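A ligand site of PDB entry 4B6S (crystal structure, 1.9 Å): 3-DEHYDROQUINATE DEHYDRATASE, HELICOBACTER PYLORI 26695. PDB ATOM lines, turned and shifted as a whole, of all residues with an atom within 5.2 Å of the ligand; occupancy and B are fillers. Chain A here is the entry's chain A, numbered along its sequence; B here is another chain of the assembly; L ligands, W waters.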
ATOM      1  N   PRO A   9      31.758 -12.973   3.548  1.00  0.00           N
ATOM      2  CA  PRO A   9      31.571 -14.403   3.756  1.00  0.00           C
ATOM      3  C   PRO A   9      30.282 -14.982   3.140  1.00  0.00           C
ATOM      4  O   PRO A   9      29.241 -14.345   3.173  1.00  0.00           O
ATOM      5  CB  PRO A   9      31.570 -14.551   5.305  1.00  0.00           C
ATOM      6  CG  PRO A   9      31.262 -13.179   5.794  1.00  0.00           C
ATOM      7  CD  PRO A   9      31.865 -12.241   4.823  1.00  0.00           C
ATOM      8  N   ASN A  10      30.407 -16.176   2.569  1.00  0.00           N
ATOM      9  CA  ASN A  10      29.301 -16.949   1.983  1.00  0.00           C
ATOM     10  C   ASN A  10      28.776 -16.453   0.642  1.00  0.00           C
ATOM     11  O   ASN A  10      27.950 -17.120   0.049  1.00  0.00           O
ATOM     12  CB  ASN A  10      28.149 -17.136   2.999  1.00  0.00           C
ATOM     13  CG  ASN A  10      28.585 -17.903   4.229  1.00  0.00           C
ATOM     14  OD1 ASN A  10      29.150 -18.981   4.122  1.00  0.00           O
ATOM     15  ND2 ASN A  10      28.375 -17.323   5.399  1.00  0.00           N
ATOM     16  N   LEU A  11      29.252 -15.306   0.161  1.00  0.00           N
ATOM     17  CA  LEU A  11      28.798 -14.742  -1.120  1.00  0.00           C
ATOM     18  C   LEU A  11      29.202 -15.636  -2.264  1.00  0.00           C
ATOM     19  O   LEU A  11      28.519 -15.706  -3.296  1.00  0.00           O
ATOM     20  CB  LEU A  11      29.343 -13.344  -1.344  1.00  0.00           C
ATOM     21  CG  LEU A  11      28.459 -12.157  -0.909  1.00  0.00           C
ATOM     22  CD1 LEU A  11      27.140 -12.159  -1.705  1.00  0.00           C
ATOM     23  CD2 LEU A  11      28.170 -12.144   0.529  1.00  0.00           C
ATOM     24  N   MET A  13      28.763 -18.664  -2.216  1.00  0.00           N
ATOM     25  CA  MET A  13      27.806 -19.766  -2.234  1.00  0.00           C
ATOM     26  C   MET A  13      26.497 -19.488  -2.950  1.00  0.00           C
ATOM     27  O   MET A  13      25.597 -20.336  -2.957  1.00  0.00           O
ATOM     28  CB  MET A  13      27.496 -20.255  -0.826  1.00  0.00           C
ATOM     29  CG  MET A  13      28.732 -20.685  -0.069  1.00  0.00           C
ATOM     30  SD  MET A  13      29.768 -22.028  -0.768  1.00  0.00           S
ATOM     31  CE  MET A  13      28.861 -23.541  -0.407  1.00  0.00           C
ATOM     32  N   LEU A  14      26.396 -18.299  -3.527  1.00  0.00           N
ATOM     33  CA  LEU A  14      25.254 -17.901  -4.387  1.00  0.00           C
ATOM     34  C   LEU A  14      25.022 -18.855  -5.537  1.00  0.00           C
ATOM     35  O   LEU A  14      25.949 -19.193  -6.258  1.00  0.00           O
ATOM     36  CB  LEU A  14      25.527 -16.562  -5.023  1.00  0.00           C
ATOM     37  CG  LEU A  14      25.257 -15.380  -4.127  1.00  0.00           C
ATOM     38  CD1 LEU A  14      25.883 -14.204  -4.797  1.00  0.00           C
ATOM     39  CD2 LEU A  14      23.745 -15.187  -3.946  1.00  0.00           C
ATOM     40  N   TYR A  22      17.960 -15.690  -1.859  1.00  0.00           N
ATOM     41  CA  TYR A  22      18.909 -15.147  -2.834  1.00  0.00           C
ATOM     42  C   TYR A  22      18.464 -15.643  -4.237  1.00  0.00           C
ATOM     43  O   TYR A  22      17.293 -15.999  -4.429  1.00  0.00           O
ATOM     44  CB  TYR A  22      20.359 -15.477  -2.421  1.00  0.00           C
ATOM     45  CG  TYR A  22      20.537 -15.383  -0.906  1.00  0.00           C
ATOM     46  CD1 TYR A  22      20.290 -14.183  -0.228  1.00  0.00           C
ATOM     47  CD2 TYR A  22      20.874 -16.508  -0.135  1.00  0.00           C
ATOM     48  CE1 TYR A  22      20.393 -14.091   1.184  1.00  0.00           C
ATOM     49  CE2 TYR A  22      20.977 -16.427   1.286  1.00  0.00           C
ATOM     50  CZ  TYR A  22      20.731 -15.203   1.927  1.00  0.00           C
ATOM     51  OH  TYR A  22      20.834 -15.076   3.303  1.00  0.00           O
ATOM     52  N   ASN A  76      30.252  -5.807  -0.318  1.00  0.00           N
ATOM     53  CA  ASN A  76      29.205  -6.507   0.418  1.00  0.00           C
ATOM     54  C   ASN A  76      29.915  -7.321   1.528  1.00  0.00           C
ATOM     55  O   ASN A  76      30.440  -8.356   1.238  1.00  0.00           O
ATOM     56  CB  ASN A  76      28.410  -7.438  -0.522  1.00  0.00           C
ATOM     57  CG  ASN A  76      27.229  -8.159   0.173  1.00  0.00           C
ATOM     58  OD1 ASN A  76      27.147  -8.269   1.420  1.00  0.00           O
ATOM     59  ND2 ASN A  76      26.291  -8.640  -0.625  1.00  0.00           N
ATOM     60  N   PRO A  77      29.941  -6.817   2.782  1.00  0.00           N
ATOM     61  CA  PRO A  77      30.659  -7.513   3.848  1.00  0.00           C
ATOM     62  C   PRO A  77      29.911  -8.698   4.398  1.00  0.00           C
ATOM     63  O   PRO A  77      30.404  -9.356   5.284  1.00  0.00           O
ATOM     64  CB  PRO A  77      30.823  -6.451   4.921  1.00  0.00           C
ATOM     65  CG  PRO A  77      30.620  -5.240   4.252  1.00  0.00           C
ATOM     66  CD  PRO A  77      29.618  -5.471   3.204  1.00  0.00           C
ATOM     67  N   GLY A  78      28.734  -8.999   3.866  1.00  0.00           N
ATOM     68  CA  GLY A  78      28.097 -10.259   4.259  1.00  0.00           C
ATOM     69  C   GLY A  78      27.669 -10.121   5.725  1.00  0.00           C
ATOM     70  O   GLY A  78      27.280  -9.043   6.143  1.00  0.00           O
ATOM     71  N   ALA A  79      27.771 -11.199   6.500  1.00  0.00           N
ATOM     72  CA  ALA A  79      27.376 -11.141   7.909  1.00  0.00           C
ATOM     73  C   ALA A  79      28.290 -10.242   8.781  1.00  0.00           C
ATOM     74  O   ALA A  79      27.861  -9.774   9.843  1.00  0.00           O
ATOM     75  CB  ALA A  79      27.270 -12.567   8.496  1.00  0.00           C
ATOM     76  N   SER A  81      28.942  -7.320   8.106  1.00  0.00           N
ATOM     77  CA  SER A  81      28.303  -5.983   8.147  1.00  0.00           C
ATOM     78  C   SER A  81      27.791  -5.648   9.536  1.00  0.00           C
ATOM     79  O   SER A  81      27.924  -4.486  10.008  1.00  0.00           O
ATOM     80  CB  SER A  81      27.092  -5.915   7.181  1.00  0.00           C
ATOM     81  OG  SER A  81      27.504  -6.203   5.845  1.00  0.00           O
ATOM     82  N   HIS A  82      27.192  -6.652  10.183  1.00  0.00           N
ATOM     83  CA  HIS A  82      26.455  -6.465  11.409  1.00  0.00           C
ATOM     84  C   HIS A  82      27.357  -6.527  12.627  1.00  0.00           C
ATOM     85  O   HIS A  82      26.987  -6.048  13.689  1.00  0.00           O
ATOM     86  CB  HIS A  82      25.337  -7.503  11.550  1.00  0.00           C
ATOM     87  CG  HIS A  82      24.635  -7.816  10.268  1.00  0.00           C
ATOM     88  ND1 HIS A  82      23.887  -6.891   9.586  1.00  0.00           N
ATOM     89  CD2 HIS A  82      24.571  -8.958   9.544  1.00  0.00           C
ATOM     90  CE1 HIS A  82      23.412  -7.435   8.478  1.00  0.00           C
ATOM     91  NE2 HIS A  82      23.814  -8.694   8.425  1.00  0.00           N
ATOM     92  N   VAL A 101      26.781  -2.786  -0.589  1.00  0.00           N
ATOM     93  CA  VAL A 101      25.685  -3.452  -1.291  1.00  0.00           C
ATOM     94  C   VAL A 101      25.239  -4.670  -0.479  1.00  0.00           C
ATOM     95  O   VAL A 101      26.082  -5.421   0.006  1.00  0.00           O
ATOM     96  CB  VAL A 101      26.083  -4.013  -2.687  1.00  0.00           C
ATOM     97  CG1 VAL A 101      24.931  -4.790  -3.309  1.00  0.00           C
ATOM     98  CG2 VAL A 101      26.543  -2.920  -3.646  1.00  0.00           C
ATOM     99  N   HIS A 102      23.916  -4.853  -0.363  1.00  0.00           N
ATOM    100  CA  HIS A 102      23.345  -6.115   0.069  1.00  0.00           C
ATOM    101  C   HIS A 102      22.367  -6.621  -0.962  1.00  0.00           C
ATOM    102  O   HIS A 102      21.617  -5.841  -1.542  1.00  0.00           O
ATOM    103  CB  HIS A 102      22.650  -5.935   1.422  1.00  0.00           C
ATOM    104  CG  HIS A 102      23.564  -5.456   2.491  1.00  0.00           C
ATOM    105  ND1 HIS A 102      24.431  -6.285   3.163  1.00  0.00           N
ATOM    106  CD2 HIS A 102      23.781  -4.220   2.994  1.00  0.00           C
ATOM    107  CE1 HIS A 102      25.135  -5.589   4.028  1.00  0.00           C
ATOM    108  NE2 HIS A 102      24.755  -4.332   3.951  1.00  0.00           N
ATOM    109  N   LEU A 103      22.376  -7.923  -1.208  1.00  0.00           N
ATOM    110  CA  LEU A 103      21.372  -8.531  -2.093  1.00  0.00           C
ATOM    111  C   LEU A 103      19.993  -8.379  -1.491  1.00  0.00           C
ATOM    112  O   LEU A 103      19.032  -8.046  -2.192  1.00  0.00           O
ATOM    113  CB  LEU A 103      21.682 -10.010  -2.352  1.00  0.00           C
ATOM    114  CG  LEU A 103      23.017 -10.328  -3.013  1.00  0.00           C
ATOM    115  CD1 LEU A 103      23.169 -11.848  -3.085  1.00  0.00           C
ATOM    116  CD2 LEU A 103      23.026  -9.775  -4.414  1.00  0.00           C
ATOM    117  N   THR A 104      19.901  -8.549  -0.182  1.00  0.00           N
ATOM    118  CA  THR A 104      18.621  -8.587   0.458  1.00  0.00           C
ATOM    119  C   THR A 104      18.403  -7.293   1.174  1.00  0.00           C
ATOM    120  O   THR A 104      19.344  -6.511   1.381  1.00  0.00           O
ATOM    121  CB  THR A 104      18.472  -9.787   1.447  1.00  0.00           C
ATOM    122  OG1 THR A 104      19.444  -9.686   2.503  1.00  0.00           O
ATOM    123  CG2 THR A 104      18.658 -11.116   0.712  1.00  0.00           C
ATOM    124  N   ILE A 106      18.096  -5.615   4.414  1.00  0.00           N
ATOM    125  CA  ILE A 106      18.474  -5.948   5.787  1.00  0.00           C
ATOM    126  C   ILE A 106      17.637  -5.283   6.870  1.00  0.00           C
ATOM    127  O   ILE A 106      17.812  -5.624   8.051  1.00  0.00           O
ATOM    128  CB  ILE A 106      19.998  -5.810   6.070  1.00  0.00           C
ATOM    129  CG1 ILE A 106      20.525  -4.394   5.745  1.00  0.00           C
ATOM    130  CG2 ILE A 106      20.741  -6.862   5.278  1.00  0.00           C
ATOM    131  CD1 ILE A 106      21.839  -3.995   6.461  1.00  0.00           C
ATOM    132  N   ARG A 109      14.446  -8.384   7.736  1.00  0.00           N
ATOM    133  CA  ARG A 109      14.768  -9.753   8.095  1.00  0.00           C
ATOM    134  C   ARG A 109      14.906  -9.779   9.608  1.00  0.00           C
ATOM    135  O   ARG A 109      14.249  -9.006  10.293  1.00  0.00           O
ATOM    136  CB  ARG A 109      16.047 -10.207   7.357  1.00  0.00           C
ATOM    137  CG  ARG A 109      16.038  -9.872   5.862  1.00  0.00           C
ATOM    138  CD  ARG A 109      17.196 -10.489   5.095  1.00  0.00           C
ATOM    139  NE  ARG A 109      17.349 -11.891   5.457  1.00  0.00           N
ATOM    140  CZ  ARG A 109      18.311 -12.682   5.005  1.00  0.00           C
ATOM    141  NH1 ARG A 109      19.241 -12.230   4.178  1.00  0.00           N
ATOM    142  NH2 ARG A 109      18.357 -13.926   5.414  1.00  0.00           N
ATOM    143  N   ARG A 113      20.200  -8.553  11.891  1.00  0.00           N
ATOM    144  CA  ARG A 113      20.729  -8.050  10.637  1.00  0.00           C
ATOM    145  C   ARG A 113      20.541  -6.539  10.438  1.00  0.00           C
ATOM    146  O   ARG A 113      21.098  -5.973   9.513  1.00  0.00           O
ATOM    147  CB  ARG A 113      20.120  -8.781   9.414  1.00  0.00           C
ATOM    148  CG  ARG A 113      20.368 -10.247   9.393  1.00  0.00           C
ATOM    149  CD  ARG A 113      20.053 -10.874   8.021  1.00  0.00           C
ATOM    150  NE  ARG A 113      19.973 -12.356   8.135  1.00  0.00           N
ATOM    151  CZ  ARG A 113      20.991 -13.216   8.039  1.00  0.00           C
ATOM    152  NH1 ARG A 113      22.228 -12.819   7.787  1.00  0.00           N
ATOM    153  NH2 ARG A 113      20.767 -14.505   8.200  1.00  0.00           N
ATOM    154  N   ILE B  85      27.468 -14.589  13.141  1.00  0.00           N
ATOM    155  CA  ILE B  85      26.381 -14.641  12.176  1.00  0.00           C
ATOM    156  C   ILE B  85      26.872 -15.320  10.900  1.00  0.00           C
ATOM    157  O   ILE B  85      26.097 -16.003  10.261  1.00  0.00           O
ATOM    158  CB  ILE B  85      25.771 -13.194  11.920  1.00  0.00           C
ATOM    159  CG1 ILE B  85      25.226 -12.602  13.238  1.00  0.00           C
ATOM    160  CG2 ILE B  85      24.701 -13.202  10.863  1.00  0.00           C
ATOM    161  CD1 ILE B  85      24.872 -11.051  13.134  1.00  0.00           C
ATOM    162  N   ASP B  89      25.291 -18.503   9.046  1.00  0.00           N
ATOM    163  CA  ASP B  89      24.807 -18.434   7.653  1.00  0.00           C
ATOM    164  C   ASP B  89      25.377 -19.634   6.888  1.00  0.00           C
ATOM    165  O   ASP B  89      24.690 -20.279   6.052  1.00  0.00           O
ATOM    166  CB  ASP B  89      25.270 -17.162   6.932  1.00  0.00           C
ATOM    167  CG  ASP B  89      24.444 -15.873   7.286  1.00  0.00           C
ATOM    168  OD1 ASP B  89      23.335 -15.930   7.837  1.00  0.00           O
ATOM    169  OD2 ASP B  89      24.909 -14.783   6.929  1.00  0.00           O
ATOM    170  N   ALA B  90      26.649 -19.921   7.149  1.00  0.00           N
ATOM    171  CA  ALA B  90      27.297 -21.108   6.580  1.00  0.00           C
ATOM    172  C   ALA B  90      26.572 -22.406   6.985  1.00  0.00           C
ATOM    173  O   ALA B  90      26.236 -23.217   6.126  1.00  0.00           O
ATOM    174  CB  ALA B  90      28.789 -21.135   6.918  1.00  0.00           C
ATOM    175  N   LEU B  93      23.331 -23.124   5.059  1.00  0.00           N
ATOM    176  CA  LEU B  93      23.408 -23.489   3.655  1.00  0.00           C
ATOM    177  C   LEU B  93      24.143 -24.796   3.500  1.00  0.00           C
ATOM    178  O   LEU B  93      24.393 -25.242   2.384  1.00  0.00           O
ATOM    179  CB  LEU B  93      24.047 -22.366   2.827  1.00  0.00           C
ATOM    180  CG  LEU B  93      25.423 -21.781   3.160  1.00  0.00           C
ATOM    181  CD1 LEU B  93      26.598 -22.728   2.829  1.00  0.00           C
ATOM    182  CD2 LEU B  93      25.598 -20.463   2.456  1.00  0.00           C
HETATM  183  F1  LIG L   1      24.185 -13.357  -0.407  1.00  0.00           F
HETATM  184  C1  LIG L   1      24.222 -14.267   0.586  1.00  0.00           C
HETATM  185  C2  LIG L   1      24.667 -15.541   0.282  1.00  0.00           C
HETATM  186  F2  LIG L   1      25.047 -15.857  -0.950  1.00  0.00           F
HETATM  187  C3  LIG L   1      24.743 -16.521   1.240  1.00  0.00           C
HETATM  188  F3  LIG L   1      25.175 -17.738   0.952  1.00  0.00           F
HETATM  189  C4  LIG L   1      24.377 -16.219   2.524  1.00  0.00           C
HETATM  190  F4  LIG L   1      24.454 -17.174   3.444  1.00  0.00           F
HETATM  191  C5  LIG L   1      23.924 -14.956   2.825  1.00  0.00           C
HETATM  192  F5  LIG L   1      23.579 -14.760   4.097  1.00  0.00           F
HETATM  193  C6  LIG L   1      23.828 -13.930   1.880  1.00  0.00           C
HETATM  194  C7  LIG L   1      23.293 -12.510   2.201  1.00  0.00           C
HETATM  195  C8  LIG L   1      24.366 -11.512   2.629  1.00  0.00           C
HETATM  196  C9  LIG L   1      23.860 -10.073   2.814  1.00  0.00           C
HETATM  197  O1  LIG L   1      24.954  -9.185   2.976  1.00  0.00           O
HETATM  198  C10 LIG L   1      23.179  -9.724   1.513  1.00  0.00           C
HETATM  199  O2  LIG L   1      23.914  -9.500   0.556  1.00  0.00           O
HETATM  200  O3  LIG L   1      21.946  -9.663   1.512  1.00  0.00           O
HETATM  201  C11 LIG L   1      24.833 -11.979   3.976  1.00  0.00           C
HETATM  202  O4  LIG L   1      25.919 -12.561   3.988  1.00  0.00           O
HETATM  203  C12 LIG L   1      23.979 -11.747   5.243  1.00  0.00           C
HETATM  204  O5  LIG L   1      24.610 -12.275   6.411  1.00  0.00           O
HETATM  205  C13 LIG L   1      23.602 -10.275   5.359  1.00  0.00           C
HETATM  206  O6  LIG L   1      22.643 -10.161   6.391  1.00  0.00           O
HETATM  207  C14 LIG L   1      22.912  -9.893   4.020  1.00  0.00           C
HETATM  208  O   HOH W   1      21.665 -16.897   5.689  1.00  0.00           O
HETATM  209  O   HOH W   2      22.513 -19.394  -0.184  1.00  0.00           O
HETATM  210  O   HOH W   3      27.742 -14.355   5.621  1.00  0.00           O
HETATM  211  O   HOH W   4      22.546 -19.224   4.530  1.00  0.00           O
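N of Ala 79 lies within hydrogen-bond range of O5 of the ligand, at 3.3 Å.
The guanidinium group of Arg 113 sits at hydrogen-bond distance from an oxygen (O5) of the ligand, at 2.8 Å.
An oxygen (O3) of the ligand is in hydrogen-bond range of the backbone NH (N) of Thr 104 (2.9 Å).
A ring nitrogen (ND1) of His 102 sits at hydrogen-bond distance from an oxygen (O1) of the ligand (3.0 Å).
An oxygen (O5) of the ligand sits at hydrogen-bond distance from the side-chain carboxylate (OD2) of Asp 89 of chain B, at 2.6 Å.
NE2 of His 82 lies within hydrogen-bond range of O6 of the ligand (2.8 Å).
OG1 of Thr 104 sits at hydrogen-bond distance from O3 of the ligand.
The side-chain amide nitrogen (ND2) of Asn 76 is in hydrogen-bond range of an oxygen (O2) of the ligand, at 2.8 Å.
The backbone NH (N) of Leu 103 lies within hydrogen-bond range of an oxygen (O2) of the ligand (2.8 Å).
The guanidinium group (NH1) of Arg 109 sits at hydrogen-bond distance from the side-chain hydroxyl (OG1) of Thr 104, at 3.1 Å.
ND2 of Asn 76 lies close to O of Val 101, 3.3 Å away.
ND1 of His 82 sits close to O of Arg 113, at 2.9 Å.
The guanidinium group (NH1) of Arg 109 lies within hydrogen-bond range of the side-chain hydroxyl (OH) of Tyr 22 (3.4 Å).
The guanidinium group (NH2) of Arg 113 is in salt-bridge range of the side-chain carboxylate (OD1) of Asp 89 of chain B.
The side-chain amide oxygen of Asn 76 is in hydrogen-bond range of the backbone NH of Gly 78.
The backbone carbonyl oxygen (O) of Gly 78 sits at hydrogen-bond distance from the side-chain hydroxyl (OG) of Ser 81 (2.9 Å).
F3 of the ligand sits close to O of Asn 10, 3.0 Å away.
A fluorine (F5) of the ligand sits close to the side-chain hydroxyl (OH) of Tyr 22.
O of Pro 9 touches O4 of the ligand, 3.9 Å away.
Leu 11 touches the ligand (CD1 to F1, 3.4 Å).
Met 13 touches the ligand (CB to F3, 3.9 Å).
Leu 14 touches the ligand.
Gly 78 touches the ligand (CA to O4, 3.2 Å).
CG2 of Ile 106 touches C14 of the ligand, at 3.9 Å.
CD2 of Leu 93 of chain B touches F3 of the ligand, 3.1 Å away.
Hydrophobic or aromatic side chains that line the ligand: Leu 11, Met 13, Leu 14, Tyr 22, Ala 79, His 82, His 102, Leu 103, Ile 106 and Leu 93 of chain B.
17 residues have an atom within 4 Å of the ligand: Pro 9, Asn 10, Leu 11, Met 13, Leu 14, Tyr 22, Asn 76, Gly 78, Ala 79, His 82, His 102, Leu 103, Thr 104, Ile 106, Arg 113, Asp 89 of chain B and Leu 93 of chain B.
The nearest printed residue that does not touch the ligand is Arg 109 (4.4 Å).
Water W1 lies within hydrogen-bond range of OD1 of Asp 89 of chain B and OH of Tyr 22.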
